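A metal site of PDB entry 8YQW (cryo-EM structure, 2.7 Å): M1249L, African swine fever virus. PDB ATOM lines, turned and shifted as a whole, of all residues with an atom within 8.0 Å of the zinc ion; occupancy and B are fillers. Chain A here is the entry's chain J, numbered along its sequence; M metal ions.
Within 4 Å of the zinc ion: Cys 937, His 943, Cys 950 and Cys 953.
The nearest printed residue that does not touch the zinc ion is Pro 938 (4.3 Å).
The zinc ion is bound by ND1 of His 943 (2.1 Å), SG of Cys 953 (2.3 Å), SG of Cys 950 (2.3 Å) and SG of Cys 937 (2.3 Å).
The backbone NH (N) of Lys 952 sits close to the side-chain sulfur (SG) of Cys 950.
SG of Cys 950 sits close to N of Asp 944, 3.3 Å away.
The side-chain sulfur of Cys 953 lies close to the backbone NH of Leu 955 (3.6 Å).
The backbone carbonyl oxygen (O) of Leu 955 is in hydrogen-bond range of the backbone NH (N) of Cys 950 (3.0 Å).
The backbone carbonyl oxygen (O) of Tyr 933 sits at hydrogen-bond distance from a ring nitrogen (NE2) of His 943 (3.4 Å).
The backbone carbonyl oxygen (O) of Arg 936 sits at hydrogen-bond distance from a ring nitrogen (NE2) of His 943.
The backbone NH (N) of His 943 is in hydrogen-bond range of the backbone carbonyl oxygen (O) of Ser 935, at 3.0 Å.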
ATOM      1  N   TYR A 933     -15.061   3.450   7.564  1.00  0.00           N
ATOM      2  CA  TYR A 933     -15.434   2.100   7.968  1.00  0.00           C
ATOM      3  C   TYR A 933     -15.366   1.927   9.484  1.00  0.00           C
ATOM      4  O   TYR A 933     -14.762   0.995  10.000  1.00  0.00           O
ATOM      5  CB  TYR A 933     -14.552   1.078   7.263  1.00  0.00           C
ATOM      6  CG  TYR A 933     -14.836   0.962   5.784  1.00  0.00           C
ATOM      7  CD1 TYR A 933     -16.137   0.964   5.309  1.00  0.00           C
ATOM      8  CD2 TYR A 933     -13.803   0.851   4.865  1.00  0.00           C
ATOM      9  CE1 TYR A 933     -16.409   0.853   3.964  1.00  0.00           C
ATOM     10  CE2 TYR A 933     -14.062   0.739   3.515  1.00  0.00           C
ATOM     11  CZ  TYR A 933     -15.367   0.737   3.068  1.00  0.00           C
ATOM     12  OH  TYR A 933     -15.622   0.629   1.726  1.00  0.00           O
ATOM     13  N   GLU A 934     -16.010   2.846  10.207  1.00  0.00           N
ATOM     14  CA  GLU A 934     -16.127   2.741  11.651  1.00  0.00           C
ATOM     15  C   GLU A 934     -17.377   1.963  12.034  1.00  0.00           C
ATOM     16  O   GLU A 934     -17.309   0.955  12.743  1.00  0.00           O
ATOM     17  CB  GLU A 934     -16.136   4.140  12.284  1.00  0.00           C
ATOM     18  CG  GLU A 934     -16.161   4.127  13.788  1.00  0.00           C
ATOM     19  CD  GLU A 934     -16.171   5.522  14.376  1.00  0.00           C
ATOM     20  OE1 GLU A 934     -16.225   6.498  13.594  1.00  0.00           O
ATOM     21  OE2 GLU A 934     -16.106   5.651  15.611  1.00  0.00           O
ATOM     22  N   SER A 935     -18.535   2.436  11.576  1.00  0.00           N
ATOM     23  CA  SER A 935     -19.790   1.705  11.645  1.00  0.00           C
ATOM     24  C   SER A 935     -20.143   1.032  10.334  1.00  0.00           C
ATOM     25  O   SER A 935     -20.658  -0.088  10.327  1.00  0.00           O
ATOM     26  CB  SER A 935     -20.926   2.634  12.064  1.00  0.00           C
ATOM     27  OG  SER A 935     -20.652   3.255  13.302  1.00  0.00           O
ATOM     28  N   ARG A 936     -19.878   1.712   9.211  1.00  0.00           N
ATOM     29  CA  ARG A 936     -20.184   1.155   7.910  1.00  0.00           C
ATOM     30  C   ARG A 936     -19.364  -0.097   7.656  1.00  0.00           C
ATOM     31  O   ARG A 936     -18.162  -0.134   7.941  1.00  0.00           O
ATOM     32  CB  ARG A 936     -19.890   2.198   6.819  1.00  0.00           C
ATOM     33  CG  ARG A 936     -20.800   3.409   6.883  1.00  0.00           C
ATOM     34  CD  ARG A 936     -20.532   4.397   5.757  1.00  0.00           C
ATOM     35  NE  ARG A 936     -19.729   5.528   6.228  1.00  0.00           N
ATOM     36  CZ  ARG A 936     -20.172   6.772   6.314  1.00  0.00           C
ATOM     37  NH1 ARG A 936     -21.401   7.099   5.953  1.00  0.00           N
ATOM     38  NH2 ARG A 936     -19.350   7.711   6.770  1.00  0.00           N
ATOM     39  N   CYS A 937     -20.012  -1.136   7.147  1.00  0.00           N
ATOM     40  CA  CYS A 937     -19.294  -2.375   6.883  1.00  0.00           C
ATOM     41  C   CYS A 937     -18.977  -2.483   5.405  1.00  0.00           C
ATOM     42  O   CYS A 937     -19.840  -2.176   4.568  1.00  0.00           O
ATOM     43  CB  CYS A 937     -20.124  -3.579   7.320  1.00  0.00           C
ATOM     44  SG  CYS A 937     -19.178  -5.084   7.601  1.00  0.00           S
ATOM     45  N   PRO A 938     -17.757  -2.870   5.030  1.00  0.00           N
ATOM     46  CA  PRO A 938     -17.452  -3.069   3.610  1.00  0.00           C
ATOM     47  C   PRO A 938     -18.301  -4.156   2.962  1.00  0.00           C
ATOM     48  O   PRO A 938     -18.468  -4.145   1.741  1.00  0.00           O
ATOM     49  CB  PRO A 938     -15.968  -3.434   3.608  1.00  0.00           C
ATOM     50  CG  PRO A 938     -15.449  -2.894   4.897  1.00  0.00           C
ATOM     51  CD  PRO A 938     -16.564  -3.039   5.876  1.00  0.00           C
ATOM     52  N   LYS A 939     -18.827  -5.091   3.747  1.00  0.00           N
ATOM     53  CA  LYS A 939     -19.637  -6.175   3.223  1.00  0.00           C
ATOM     54  C   LYS A 939     -21.129  -5.834   3.192  1.00  0.00           C
ATOM     55  O   LYS A 939     -21.934  -6.695   2.858  1.00  0.00           O
ATOM     56  CB  LYS A 939     -19.413  -7.442   4.044  1.00  0.00           C
ATOM     57  CG  LYS A 939     -17.960  -7.874   4.121  1.00  0.00           C
ATOM     58  CD  LYS A 939     -17.385  -8.090   2.737  1.00  0.00           C
ATOM     59  CE  LYS A 939     -17.553  -9.537   2.296  1.00  0.00           C
ATOM     60  NZ  LYS A 939     -16.535 -10.428   2.912  1.00  0.00           N
ATOM     61  N   GLY A 940     -21.492  -4.610   3.537  1.00  0.00           N
ATOM     62  CA  GLY A 940     -22.872  -4.163   3.468  1.00  0.00           C
ATOM     63  C   GLY A 940     -23.455  -3.983   4.861  1.00  0.00           C
ATOM     64  O   GLY A 940     -23.168  -4.755   5.780  1.00  0.00           O
ATOM     65  N   GLY A 941     -24.279  -2.949   5.005  1.00  0.00           N
ATOM     66  CA  GLY A 941     -24.856  -2.671   6.303  1.00  0.00           C
ATOM     67  C   GLY A 941     -23.819  -2.164   7.281  1.00  0.00           C
ATOM     68  O   GLY A 941     -22.765  -1.628   6.916  1.00  0.00           O
ATOM     69  N   LEU A 942     -24.126  -2.335   8.565  1.00  0.00           N
ATOM     70  CA  LEU A 942     -23.228  -1.955   9.637  1.00  0.00           C
ATOM     71  C   LEU A 942     -22.487  -3.186  10.162  1.00  0.00           C
ATOM     72  O   LEU A 942     -22.835  -4.328   9.858  1.00  0.00           O
ATOM     73  CB  LEU A 942     -23.989  -1.267  10.765  1.00  0.00           C
ATOM     74  CG  LEU A 942     -24.858  -0.084  10.339  1.00  0.00           C
ATOM     75  CD1 LEU A 942     -25.505   0.579  11.536  1.00  0.00           C
ATOM     76  CD2 LEU A 942     -24.038   0.925   9.548  1.00  0.00           C
ATOM     77  N   HIS A 943     -21.451  -2.926  10.948  1.00  0.00           N
ATOM     78  CA  HIS A 943     -20.603  -4.000  11.449  1.00  0.00           C
ATOM     79  C   HIS A 943     -21.354  -4.877  12.445  1.00  0.00           C
ATOM     80  O   HIS A 943     -22.230  -4.417  13.172  1.00  0.00           O
ATOM     81  CB  HIS A 943     -19.349  -3.425  12.114  1.00  0.00           C
ATOM     82  CG  HIS A 943     -18.376  -2.819  11.162  1.00  0.00           C
ATOM     83  ND1 HIS A 943     -17.810  -3.537  10.131  1.00  0.00           N
ATOM     84  CD2 HIS A 943     -17.866  -1.570  11.076  1.00  0.00           C
ATOM     85  CE1 HIS A 943     -16.988  -2.755   9.455  1.00  0.00           C
ATOM     86  NE2 HIS A 943     -17.010  -1.554  10.008  1.00  0.00           N
ATOM     87  N   ASP A 944     -20.998  -6.158  12.461  1.00  0.00           N
ATOM     88  CA  ASP A 944     -21.563  -7.138  13.378  1.00  0.00           C
ATOM     89  C   ASP A 944     -20.412  -7.621  14.269  1.00  0.00           C
ATOM     90  O   ASP A 944     -19.788  -8.646  13.993  1.00  0.00           O
ATOM     91  CB  ASP A 944     -22.228  -8.288  12.633  1.00  0.00           C
ATOM     92  CG  ASP A 944     -22.678  -9.407  13.554  1.00  0.00           C
ATOM     93  OD1 ASP A 944     -23.380  -9.127  14.538  1.00  0.00           O
ATOM     94  OD2 ASP A 944     -22.303 -10.574  13.284  1.00  0.00           O
ATOM     95  N   PHE A 945     -20.169  -6.886  15.349  1.00  0.00           N
ATOM     96  CA  PHE A 945     -18.973  -7.081  16.171  1.00  0.00           C
ATOM     97  C   PHE A 945     -19.222  -8.212  17.165  1.00  0.00           C
ATOM     98  O   PHE A 945     -20.073  -8.093  18.062  1.00  0.00           O
ATOM     99  CB  PHE A 945     -18.617  -5.785  16.896  1.00  0.00           C
ATOM    100  CG  PHE A 945     -17.880  -4.803  16.035  1.00  0.00           C
ATOM    101  CD1 PHE A 945     -16.709  -5.169  15.399  1.00  0.00           C
ATOM    102  CD2 PHE A 945     -18.349  -3.513  15.875  1.00  0.00           C
ATOM    103  CE1 PHE A 945     -16.019  -4.270  14.619  1.00  0.00           C
ATOM    104  CE2 PHE A 945     -17.666  -2.607  15.095  1.00  0.00           C
ATOM    105  CZ  PHE A 945     -16.494  -2.986  14.464  1.00  0.00           C
ATOM    106  N   LYS A 949     -14.330  -8.757  16.895  1.00  0.00           N
ATOM    107  CA  LYS A 949     -14.086  -8.835  15.458  1.00  0.00           C
ATOM    108  C   LYS A 949     -15.415  -8.929  14.732  1.00  0.00           C
ATOM    109  O   LYS A 949     -16.270  -9.760  15.090  1.00  0.00           O
ATOM    110  CB  LYS A 949     -13.208 -10.036  15.120  1.00  0.00           C
ATOM    111  CG  LYS A 949     -12.896 -10.203  13.648  1.00  0.00           C
ATOM    112  CD  LYS A 949     -11.997 -11.405  13.430  1.00  0.00           C
ATOM    113  CE  LYS A 949     -11.680 -11.609  11.961  1.00  0.00           C
ATOM    114  NZ  LYS A 949     -10.775 -12.776  11.749  1.00  0.00           N
ATOM    115  N   CYS A 950     -15.605  -8.098  13.708  1.00  0.00           N
ATOM    116  CA  CYS A 950     -16.801  -8.194  12.892  1.00  0.00           C
ATOM    117  C   CYS A 950     -16.865  -9.555  12.214  1.00  0.00           C
ATOM    118  O   CYS A 950     -15.847 -10.099  11.772  1.00  0.00           O
ATOM    119  CB  CYS A 950     -16.837  -7.078  11.848  1.00  0.00           C
ATOM    120  SG  CYS A 950     -18.282  -7.093  10.769  1.00  0.00           S
ATOM    121  N   VAL A 951     -18.067 -10.130  12.175  1.00  0.00           N
ATOM    122  CA  VAL A 951     -18.250 -11.424  11.505  1.00  0.00           C
ATOM    123  C   VAL A 951     -18.144 -11.264   9.993  1.00  0.00           C
ATOM    124  O   VAL A 951     -17.535 -12.089   9.312  1.00  0.00           O
ATOM    125  CB  VAL A 951     -19.597 -12.043  11.927  1.00  0.00           C
ATOM    126  CG1 VAL A 951     -19.908 -13.261  11.075  1.00  0.00           C
ATOM    127  CG2 VAL A 951     -19.554 -12.424  13.395  1.00  0.00           C
ATOM    128  N   LYS A 952     -18.747 -10.207   9.442  1.00  0.00           N
ATOM    129  CA  LYS A 952     -18.828 -10.056   8.002  1.00  0.00           C
ATOM    130  C   LYS A 952     -17.463  -9.763   7.381  1.00  0.00           C
ATOM    131  O   LYS A 952     -17.086 -10.370   6.379  1.00  0.00           O
ATOM    132  CB  LYS A 952     -19.831  -8.957   7.648  1.00  0.00           C
ATOM    133  CG  LYS A 952     -21.201  -9.156   8.288  1.00  0.00           C
ATOM    134  CD  LYS A 952     -22.271  -8.363   7.562  1.00  0.00           C
ATOM    135  CE  LYS A 952     -22.274  -6.901   7.986  1.00  0.00           C
ATOM    136  NZ  LYS A 952     -22.879  -6.716   9.339  1.00  0.00           N
ATOM    137  N   CYS A 953     -16.718  -8.834   7.981  1.00  0.00           N
ATOM    138  CA  CYS A 953     -15.386  -8.469   7.494  1.00  0.00           C
ATOM    139  C   CYS A 953     -14.358  -8.812   8.561  1.00  0.00           C
ATOM    140  O   CYS A 953     -14.663  -9.454   9.565  1.00  0.00           O
ATOM    141  CB  CYS A 953     -15.344  -6.992   7.101  1.00  0.00           C
ATOM    142  SG  CYS A 953     -15.516  -5.822   8.463  1.00  0.00           S
ATOM    143  N   GLY A 954     -13.113  -8.404   8.339  1.00  0.00           N
ATOM    144  CA  GLY A 954     -12.046  -8.718   9.258  1.00  0.00           C
ATOM    145  C   GLY A 954     -11.676  -7.577  10.191  1.00  0.00           C
ATOM    146  O   GLY A 954     -10.534  -7.510  10.667  1.00  0.00           O
ATOM    147  N   LEU A 955     -12.614  -6.674  10.456  1.00  0.00           N
ATOM    148  CA  LEU A 955     -12.304  -5.501  11.259  1.00  0.00           C
ATOM    149  C   LEU A 955     -12.175  -5.867  12.731  1.00  0.00           C
ATOM    150  O   LEU A 955     -13.002  -6.591  13.275  1.00  0.00           O
ATOM    151  CB  LEU A 955     -13.375  -4.429  11.077  1.00  0.00           C
ATOM    152  CG  LEU A 955     -13.117  -3.141  11.849  1.00  0.00           C
ATOM    153  CD1 LEU A 955     -11.755  -2.573  11.503  1.00  0.00           C
ATOM    154  CD2 LEU A 955     -14.200  -2.114  11.587  1.00  0.00           C
ATOM    155  N   PHE A 956     -11.127  -5.353  13.371  1.00  0.00           N
ATOM    156  CA  PHE A 956     -10.914  -5.489  14.795  1.00  0.00           C
ATOM    157  C   PHE A 956     -11.261  -4.190  15.488  1.00  0.00           C
ATOM    158  O   PHE A 956     -10.996  -3.103  14.956  1.00  0.00           O
ATOM    159  CB  PHE A 956      -9.465  -5.871  15.111  1.00  0.00           C
ATOM    160  CG  PHE A 956      -9.077  -7.245  14.613  1.00  0.00           C
ATOM    161  CD1 PHE A 956      -9.536  -8.374  15.247  1.00  0.00           C
ATOM    162  CD2 PHE A 956      -8.259  -7.378  13.511  1.00  0.00           C
ATOM    163  CE1 PHE A 956      -9.176  -9.634  14.802  1.00  0.00           C
ATOM    164  CE2 PHE A 956      -7.886  -8.626  13.055  1.00  0.00           C
ATOM    165  CZ  PHE A 956      -8.351  -9.761  13.695  1.00  0.00           C
ATOM    166  N   TYR A 973      -6.139  -4.950   6.789  1.00  0.00           N
ATOM    167  CA  TYR A 973      -7.539  -4.600   6.573  1.00  0.00           C
ATOM    168  C   TYR A 973      -7.662  -3.497   5.526  1.00  0.00           C
ATOM    169  O   TYR A 973      -8.564  -3.534   4.686  1.00  0.00           O
ATOM    170  CB  TYR A 973      -8.174  -4.154   7.889  1.00  0.00           C
ATOM    171  CG  TYR A 973      -9.621  -3.760   7.779  1.00  0.00           C
ATOM    172  CD1 TYR A 973     -10.631  -4.716   7.800  1.00  0.00           C
ATOM    173  CD2 TYR A 973      -9.986  -2.424   7.659  1.00  0.00           C
ATOM    174  CE1 TYR A 973     -11.962  -4.349   7.700  1.00  0.00           C
ATOM    175  CE2 TYR A 973     -11.308  -2.047   7.563  1.00  0.00           C
ATOM    176  CZ  TYR A 973     -12.291  -3.019   7.580  1.00  0.00           C
ATOM    177  OH  TYR A 973     -13.606  -2.637   7.479  1.00  0.00           O
ATOM    178  N   TYR A 977      -9.847  -3.786   1.487  1.00  0.00           N
ATOM    179  CA  TYR A 977     -11.014  -3.044   1.026  1.00  0.00           C
ATOM    180  C   TYR A 977     -10.636  -1.637   0.558  1.00  0.00           C
ATOM    181  O   TYR A 977     -11.326  -0.673   0.879  1.00  0.00           O
ATOM    182  CB  TYR A 977     -12.068  -2.971   2.126  1.00  0.00           C
ATOM    183  CG  TYR A 977     -12.359  -4.314   2.764  1.00  0.00           C
ATOM    184  CD1 TYR A 977     -13.266  -5.201   2.189  1.00  0.00           C
ATOM    185  CD2 TYR A 977     -11.746  -4.688   3.951  1.00  0.00           C
ATOM    186  CE1 TYR A 977     -13.534  -6.414   2.769  1.00  0.00           C
ATOM    187  CE2 TYR A 977     -12.014  -5.913   4.537  1.00  0.00           C
ATOM    188  CZ  TYR A 977     -12.909  -6.763   3.940  1.00  0.00           C
ATOM    189  OH  TYR A 977     -13.177  -7.989   4.526  1.00  0.00           O
HETATM  190 ZN    ZN M   1     -17.634  -5.425   9.299  1.00  0.00          ZN
